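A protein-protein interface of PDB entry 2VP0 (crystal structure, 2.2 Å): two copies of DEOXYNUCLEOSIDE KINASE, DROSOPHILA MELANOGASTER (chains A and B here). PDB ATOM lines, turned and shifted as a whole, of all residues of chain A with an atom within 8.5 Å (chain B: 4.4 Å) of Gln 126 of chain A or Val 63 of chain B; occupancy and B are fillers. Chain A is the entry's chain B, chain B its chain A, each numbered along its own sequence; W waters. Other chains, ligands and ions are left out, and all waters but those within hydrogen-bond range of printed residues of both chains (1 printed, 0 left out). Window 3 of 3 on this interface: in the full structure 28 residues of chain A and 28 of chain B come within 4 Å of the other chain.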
ATOM      1  N   MET A  78      16.442 -20.141  25.024  1.00  0.00           N
ATOM      2  CA  MET A  78      15.391 -19.452  24.268  1.00  0.00           C
ATOM      3  C   MET A  78      14.319 -20.388  23.715  1.00  0.00           C
ATOM      4  O   MET A  78      13.125 -20.214  24.010  1.00  0.00           O
ATOM      5  CB  MET A  78      16.025 -18.668  23.129  1.00  0.00           C
ATOM      6  CG  MET A  78      15.635 -17.241  23.101  1.00  0.00           C
ATOM      7  SD  MET A  78      13.947 -16.849  22.733  1.00  0.00           S
ATOM      8  CE  MET A  78      13.598 -18.051  21.434  1.00  0.00           C
ATOM      9  N   GLU A 116      13.157 -14.249  33.583  1.00  0.00           N
ATOM     10  CA  GLU A 116      13.875 -13.133  34.213  1.00  0.00           C
ATOM     11  C   GLU A 116      15.265 -13.533  34.736  1.00  0.00           C
ATOM     12  O   GLU A 116      16.250 -12.821  34.498  1.00  0.00           O
ATOM     13  CB  GLU A 116      13.019 -12.462  35.306  1.00  0.00           C
ATOM     14  CG  GLU A 116      13.728 -11.360  36.113  1.00  0.00           C
ATOM     15  CD  GLU A 116      14.229 -10.198  35.268  1.00  0.00           C
ATOM     16  OE1 GLU A 116      13.742 -10.001  34.131  1.00  0.00           O
ATOM     17  OE2 GLU A 116      15.117  -9.470  35.755  1.00  0.00           O
ATOM     18  N   MET A 118      17.170 -15.975  33.703  1.00  0.00           N
ATOM     19  CA  MET A 118      18.022 -16.309  32.575  1.00  0.00           C
ATOM     20  C   MET A 118      18.463 -15.056  31.834  1.00  0.00           C
ATOM     21  O   MET A 118      19.538 -15.033  31.239  1.00  0.00           O
ATOM     22  CB  MET A 118      17.317 -17.290  31.636  1.00  0.00           C
ATOM     23  CG  MET A 118      17.143 -18.683  32.222  1.00  0.00           C
ATOM     24  SD  MET A 118      16.021 -19.659  31.213  1.00  0.00           S
ATOM     25  CE  MET A 118      15.991 -21.218  32.103  1.00  0.00           C
ATOM     26  N   ARG A 119      17.639 -14.014  31.879  1.00  0.00           N
ATOM     27  CA  ARG A 119      18.093 -12.703  31.425  1.00  0.00           C
ATOM     28  C   ARG A 119      19.241 -12.205  32.300  1.00  0.00           C
ATOM     29  O   ARG A 119      20.267 -11.804  31.781  1.00  0.00           O
ATOM     30  CB  ARG A 119      16.973 -11.675  31.416  1.00  0.00           C
ATOM     31  CG  ARG A 119      17.402 -10.360  30.775  1.00  0.00           C
ATOM     32  CD  ARG A 119      16.421  -9.240  31.027  1.00  0.00           C
ATOM     33  NE  ARG A 119      16.323  -8.874  32.436  1.00  0.00           N
ATOM     34  CZ  ARG A 119      17.253  -8.205  33.120  1.00  0.00           C
ATOM     35  NH1 ARG A 119      18.387  -7.828  32.535  1.00  0.00           N
ATOM     36  NH2 ARG A 119      17.047  -7.916  34.402  1.00  0.00           N
ATOM     37  N   GLY A 122      22.495 -14.101  31.851  1.00  0.00           N
ATOM     38  CA  GLY A 122      23.040 -13.993  30.496  1.00  0.00           C
ATOM     39  C   GLY A 122      22.760 -15.175  29.578  1.00  0.00           C
ATOM     40  O   GLY A 122      23.157 -15.152  28.413  1.00  0.00           O
ATOM     41  N   SER A 123      22.074 -16.200  30.089  1.00  0.00           N
ATOM     42  CA  SER A 123      21.583 -17.314  29.253  1.00  0.00           C
ATOM     43  C   SER A 123      20.717 -16.819  28.099  1.00  0.00           C
ATOM     44  O   SER A 123      20.763 -17.373  27.007  1.00  0.00           O
ATOM     45  CB  SER A 123      20.758 -18.295  30.082  1.00  0.00           C
ATOM     46  OG  SER A 123      21.537 -18.892  31.086  1.00  0.00           O
ATOM     47  N   LEU A 124      19.912 -15.791  28.364  1.00  0.00           N
ATOM     48  CA  LEU A 124      19.135 -15.119  27.330  1.00  0.00           C
ATOM     49  C   LEU A 124      19.698 -13.720  27.061  1.00  0.00           C
ATOM     50  O   LEU A 124      19.557 -12.818  27.892  1.00  0.00           O
ATOM     51  CB  LEU A 124      17.639 -15.032  27.704  1.00  0.00           C
ATOM     52  CG  LEU A 124      16.840 -16.320  27.943  1.00  0.00           C
ATOM     53  CD1 LEU A 124      15.529 -16.022  28.674  1.00  0.00           C
ATOM     54  CD2 LEU A 124      16.590 -17.102  26.638  1.00  0.00           C
ATOM     55  N   GLU A 125      20.329 -13.559  25.897  1.00  0.00           N
ATOM     56  CA  GLU A 125      20.738 -12.243  25.392  1.00  0.00           C
ATOM     57  C   GLU A 125      19.511 -11.361  25.215  1.00  0.00           C
ATOM     58  O   GLU A 125      18.391 -11.868  25.109  1.00  0.00           O
ATOM     59  CB  GLU A 125      21.447 -12.365  24.037  1.00  0.00           C
ATOM     60  CG  GLU A 125      22.508 -13.454  23.940  1.00  0.00           C
ATOM     61  CD  GLU A 125      23.920 -12.954  24.197  1.00  0.00           C
ATOM     62  OE1 GLU A 125      24.087 -11.819  24.716  1.00  0.00           O
ATOM     63  OE2 GLU A 125      24.867 -13.711  23.882  1.00  0.00           O
ATOM     64  N   GLN A 126      19.731 -10.049  25.147  1.00  0.00           N
ATOM     65  CA  GLN A 126      18.640  -9.079  25.066  1.00  0.00           C
ATOM     66  C   GLN A 126      17.604  -9.423  23.990  1.00  0.00           C
ATOM     67  O   GLN A 126      16.412  -9.447  24.265  1.00  0.00           O
ATOM     68  CB  GLN A 126      19.180  -7.654  24.854  1.00  0.00           C
ATOM     69  CG  GLN A 126      18.138  -6.572  25.106  1.00  0.00           C
ATOM     70  CD  GLN A 126      17.709  -6.505  26.563  1.00  0.00           C
ATOM     71  OE1 GLN A 126      16.526  -6.644  26.890  1.00  0.00           O
ATOM     72  NE2 GLN A 126      18.673  -6.300  27.449  1.00  0.00           N
ATOM     73  N   GLY A 127      18.075  -9.696  22.774  1.00  0.00           N
ATOM     74  CA  GLY A 127      17.217 -10.088  21.660  1.00  0.00           C
ATOM     75  C   GLY A 127      16.327 -11.284  21.946  1.00  0.00           C
ATOM     76  O   GLY A 127      15.173 -11.304  21.529  1.00  0.00           O
ATOM     77  N   MET A 128      16.859 -12.278  22.654  1.00  0.00           N
ATOM     78  CA  MET A 128      16.074 -13.473  23.004  1.00  0.00           C
ATOM     79  C   MET A 128      15.052 -13.161  24.090  1.00  0.00           C
ATOM     80  O   MET A 128      13.941 -13.702  24.098  1.00  0.00           O
ATOM     81  CB  MET A 128      16.989 -14.598  23.482  1.00  0.00           C
ATOM     82  CG  MET A 128      17.840 -15.194  22.407  1.00  0.00           C
ATOM     83  SD  MET A 128      19.235 -16.025  23.147  1.00  0.00           S
ATOM     84  CE  MET A 128      19.920 -16.858  21.714  1.00  0.00           C
ATOM     85  N   TYR A 129      15.458 -12.287  25.008  1.00  0.00           N
ATOM     86  CA  TYR A 129      14.607 -11.832  26.085  1.00  0.00           C
ATOM     87  C   TYR A 129      13.457 -11.022  25.531  1.00  0.00           C
ATOM     88  O   TYR A 129      12.305 -11.257  25.902  1.00  0.00           O
ATOM     89  CB  TYR A 129      15.401 -10.983  27.084  1.00  0.00           C
ATOM     90  CG  TYR A 129      14.516 -10.312  28.112  1.00  0.00           C
ATOM     91  CD1 TYR A 129      13.919 -11.056  29.128  1.00  0.00           C
ATOM     92  CD2 TYR A 129      14.269  -8.935  28.055  1.00  0.00           C
ATOM     93  CE1 TYR A 129      13.103 -10.453  30.067  1.00  0.00           C
ATOM     94  CE2 TYR A 129      13.450  -8.317  28.998  1.00  0.00           C
ATOM     95  CZ  TYR A 129      12.879  -9.085  30.002  1.00  0.00           C
ATOM     96  OH  TYR A 129      12.067  -8.494  30.931  1.00  0.00           O
ATOM     97  N   ASN A 130      13.790 -10.069  24.655  1.00  0.00           N
ATOM     98  CA  ASN A 130      12.816  -9.184  24.022  1.00  0.00           C
ATOM     99  C   ASN A 130      11.749  -9.938  23.237  1.00  0.00           C
ATOM    100  O   ASN A 130      10.576  -9.602  23.317  1.00  0.00           O
ATOM    101  CB  ASN A 130      13.526  -8.181  23.100  1.00  0.00           C
ATOM    102  CG  ASN A 130      14.289  -7.126  23.870  1.00  0.00           C
ATOM    103  OD1 ASN A 130      14.318  -7.141  25.102  1.00  0.00           O
ATOM    104  ND2 ASN A 130      14.913  -6.203  23.147  1.00  0.00           N
ATOM    105  N   THR A 131      12.169 -10.956  22.491  1.00  0.00           N
ATOM    106  CA  THR A 131      11.253 -11.808  21.719  1.00  0.00           C
ATOM    107  C   THR A 131      10.264 -12.532  22.634  1.00  0.00           C
ATOM    108  O   THR A 131       9.061 -12.543  22.369  1.00  0.00           O
ATOM    109  CB  THR A 131      12.041 -12.824  20.848  1.00  0.00           C
ATOM    110  OG1 THR A 131      12.906 -12.101  19.965  1.00  0.00           O
ATOM    111  CG2 THR A 131      11.100 -13.725  20.010  1.00  0.00           C
ATOM    112  N   LEU A 132      10.773 -13.133  23.708  1.00  0.00           N
ATOM    113  CA  LEU A 132       9.901 -13.793  24.694  1.00  0.00           C
ATOM    114  C   LEU A 132       8.939 -12.815  25.339  1.00  0.00           C
ATOM    115  O   LEU A 132       7.759 -13.126  25.504  1.00  0.00           O
ATOM    116  CB  LEU A 132      10.709 -14.540  25.753  1.00  0.00           C
ATOM    117  CG  LEU A 132      11.474 -15.777  25.285  1.00  0.00           C
ATOM    118  CD1 LEU A 132      12.534 -16.136  26.322  1.00  0.00           C
ATOM    119  CD2 LEU A 132      10.564 -16.980  24.984  1.00  0.00           C
ATOM    120  N   GLU A 133       9.431 -11.619  25.669  1.00  0.00           N
ATOM    121  CA  GLU A 133       8.589 -10.577  26.287  1.00  0.00           C
ATOM    122  C   GLU A 133       7.496 -10.048  25.366  1.00  0.00           C
ATOM    123  O   GLU A 133       6.360  -9.847  25.806  1.00  0.00           O
ATOM    124  CB  GLU A 133       9.443  -9.416  26.816  1.00  0.00           C
ATOM    125  CG  GLU A 133      10.057  -9.684  28.197  1.00  0.00           C
ATOM    126  CD  GLU A 133       9.022  -9.769  29.316  1.00  0.00           C
ATOM    127  OE1 GLU A 133       8.366  -8.740  29.628  1.00  0.00           O
ATOM    128  OE2 GLU A 133       8.863 -10.871  29.884  1.00  0.00           O
ATOM    129  N   ARG B  58      14.245  -5.469  12.312  1.00  0.00           N
ATOM    130  CA  ARG B  58      15.516  -4.754  12.352  1.00  0.00           C
ATOM    131  C   ARG B  58      15.668  -3.922  13.633  1.00  0.00           C
ATOM    132  O   ARG B  58      16.756  -3.427  13.921  1.00  0.00           O
ATOM    133  CB  ARG B  58      15.673  -3.838  11.129  1.00  0.00           C
ATOM    134  CG  ARG B  58      15.840  -4.542   9.799  1.00  0.00           C
ATOM    135  CD  ARG B  58      15.763  -3.553   8.639  1.00  0.00           C
ATOM    136  NE  ARG B  58      17.076  -3.237   8.080  1.00  0.00           N
ATOM    137  CZ  ARG B  58      17.293  -2.515   6.972  1.00  0.00           C
ATOM    138  NH1 ARG B  58      16.279  -1.992   6.285  1.00  0.00           N
ATOM    139  NH2 ARG B  58      18.540  -2.303   6.549  1.00  0.00           N
ATOM    140  N   ASN B  59      14.585  -3.750  14.382  1.00  0.00           N
ATOM    141  CA  ASN B  59      14.610  -2.942  15.611  1.00  0.00           C
ATOM    142  C   ASN B  59      13.553  -3.400  16.609  1.00  0.00           C
ATOM    143  O   ASN B  59      12.407  -2.986  16.534  1.00  0.00           O
ATOM    144  CB  ASN B  59      14.452  -1.444  15.274  1.00  0.00           C
ATOM    145  CG  ASN B  59      14.450  -0.519  16.530  1.00  0.00           C
ATOM    146  OD1 ASN B  59      14.516  -0.966  17.677  1.00  0.00           O
ATOM    147  ND2 ASN B  59      14.353   0.785  16.286  1.00  0.00           N
ATOM    148  N   VAL B  60      13.949  -4.279  17.524  1.00  0.00           N
ATOM    149  CA  VAL B  60      13.060  -4.783  18.562  1.00  0.00           C
ATOM    150  C   VAL B  60      13.564  -4.146  19.845  1.00  0.00           C
ATOM    151  O   VAL B  60      14.350  -4.755  20.580  1.00  0.00           O
ATOM    152  CB  VAL B  60      13.106  -6.341  18.676  1.00  0.00           C
ATOM    153  CG1 VAL B  60      12.043  -6.858  19.662  1.00  0.00           C
ATOM    154  CG2 VAL B  60      12.929  -6.993  17.310  1.00  0.00           C
ATOM    155  N   ASN B  61      13.127  -2.908  20.081  1.00  0.00           N
ATOM    156  CA  ASN B  61      13.648  -2.062  21.153  1.00  0.00           C
ATOM    157  C   ASN B  61      15.166  -1.883  21.055  1.00  0.00           C
ATOM    158  O   ASN B  61      15.886  -2.003  22.054  1.00  0.00           O
ATOM    159  CB  ASN B  61      13.246  -2.600  22.535  1.00  0.00           C
ATOM    160  CG  ASN B  61      11.742  -2.532  22.780  1.00  0.00           C
ATOM    161  OD1 ASN B  61      11.154  -1.446  22.887  1.00  0.00           O
ATOM    162  ND2 ASN B  61      11.115  -3.695  22.880  1.00  0.00           N
ATOM    163  N   GLY B  62      15.645  -1.608  19.843  1.00  0.00           N
ATOM    164  CA  GLY B  62      17.063  -1.364  19.615  1.00  0.00           C
ATOM    165  C   GLY B  62      17.873  -2.589  19.226  1.00  0.00           C
ATOM    166  O   GLY B  62      19.009  -2.457  18.778  1.00  0.00           O
ATOM    167  N   VAL B  63      17.314  -3.782  19.410  1.00  0.00           N
ATOM    168  CA  VAL B  63      17.988  -4.994  18.955  1.00  0.00           C
ATOM    169  C   VAL B  63      17.632  -5.303  17.491  1.00  0.00           C
ATOM    170  O   VAL B  63      16.458  -5.386  17.137  1.00  0.00           O
ATOM    171  CB  VAL B  63      17.707  -6.216  19.871  1.00  0.00           C
ATOM    172  CG1 VAL B  63      18.443  -7.451  19.355  1.00  0.00           C
ATOM    173  CG2 VAL B  63      18.135  -5.908  21.311  1.00  0.00           C
ATOM    174  N   ASN B  64      18.661  -5.443  16.657  1.00  0.00           N
ATOM    175  CA  ASN B  64      18.496  -5.839  15.256  1.00  0.00           C
ATOM    176  C   ASN B  64      18.513  -7.354  15.133  1.00  0.00           C
ATOM    177  O   ASN B  64      19.571  -7.945  14.979  1.00  0.00           O
ATOM    178  CB  ASN B  64      19.585  -5.202  14.365  1.00  0.00           C
ATOM    179  CG  ASN B  64      19.284  -5.332  12.853  1.00  0.00           C
ATOM    180  OD1 ASN B  64      18.576  -6.247  12.411  1.00  0.00           O
ATOM    181  ND2 ASN B  64      19.835  -4.420  12.064  1.00  0.00           N
ATOM    182  N   LEU B  65      17.337  -7.976  15.212  1.00  0.00           N
ATOM    183  CA  LEU B  65      17.236  -9.438  15.151  1.00  0.00           C
ATOM    184  C   LEU B  65      17.641 -10.006  13.786  1.00  0.00           C
ATOM    185  O   LEU B  65      18.247 -11.078  13.710  1.00  0.00           O
ATOM    186  CB  LEU B  65      15.825  -9.913  15.523  1.00  0.00           C
ATOM    187  CG  LEU B  65      15.344  -9.944  16.981  1.00  0.00           C
ATOM    188  CD1 LEU B  65      13.981 -10.635  17.055  1.00  0.00           C
ATOM    189  CD2 LEU B  65      16.363 -10.640  17.925  1.00  0.00           C
ATOM    190  N   LEU B  68      21.496 -10.132  13.594  1.00  0.00           N
ATOM    191  CA  LEU B  68      21.983 -11.236  14.424  1.00  0.00           C
ATOM    192  C   LEU B  68      21.732 -12.623  13.802  1.00  0.00           C
ATOM    193  O   LEU B  68      22.609 -13.490  13.826  1.00  0.00           O
ATOM    194  CB  LEU B  68      21.353 -11.158  15.821  1.00  0.00           C
ATOM    195  CG  LEU B  68      21.905 -10.043  16.709  1.00  0.00           C
ATOM    196  CD1 LEU B  68      20.848  -9.551  17.647  1.00  0.00           C
ATOM    197  CD2 LEU B  68      23.147 -10.529  17.480  1.00  0.00           C
HETATM  198  O   HOH W   1      16.404  -3.820  24.037  1.00  0.00           O
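The backbone carbonyl oxygen (O) of Val 60 of chain B sits at hydrogen-bond distance from the side-chain amide nitrogen (ND2) of Asn 130 of chain A, at 3.0 Å.
The side-chain amide oxygen (OD1) of Asn 130 of chain A lies close to the side-chain amide oxygen (OE1) of Gln 126 of chain A, at 2.9 Å.
The backbone carbonyl oxygen (O) of Gly 127 of chain A lies within hydrogen-bond range of the side-chain hydroxyl (OG1) of Thr 131 of chain A.
Among the printed residues, merely in contact across the chains: Thr 131 of chain A with Leu 65 of chain B, Gly 127 of chain A with Val 63 of chain B, Asn 130 of chain A with Val 63 of chain B, Gln 126 of chain A with Val 63 of chain B and Gly 127 of chain A with Leu 65 of chain B.
Gln 126 of chain A touches just one residue of chain B: Val 63.
Val 63 of chain B touches three residues of chain A.
No residue of chain A comes within 4 Å of Gly 62 of chain B.
Of the printed residues of chain B, Asn 130 of chain A touches Val 60 and Val 63.
Printed residues of chain A within 4 Å of Leu 65 of chain B: Gly 127 and Thr 131.
Of the printed residues of chain B, Thr 131 of chain A touches Leu 65.
Of the printed residues of chain A, Val 60 of chain B touches Asn 130.
Printed residues of chain B within 4 Å of Gly 127 of chain A: Val 63 and Leu 65.
Arg 119 of chain A touches none of the printed residues of chain B.
The nearest printed residue of chain B that does not touch Asn 130 of chain A is Asn 61 of chain B (4.02 Å).
Of the 9 printed residues of chain B, 3 touch a printed residue of chain A.
Printed residues of chain B that touch a printed residue of chain A: Val 60, Val 63 and Leu 65.
Hydrophobic or aromatic side chains of chain B that line the printed part of chain A: Val 60, Val 63 and Leu 65.
Among the printed residues, 6 pairs touch across the chains.
No position is printed for both chains.
Of the 6 pairs that touch across the chains among the printed residues, none has its exchanged pair printed and touching as well.
Water W1 lies within hydrogen-bond range of the backbone carbonyl oxygen (O) of Asn 61 of chain B (2.7 Å) and the side-chain amide nitrogen (ND2) of Asn 130 of chain A (2.9 Å).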
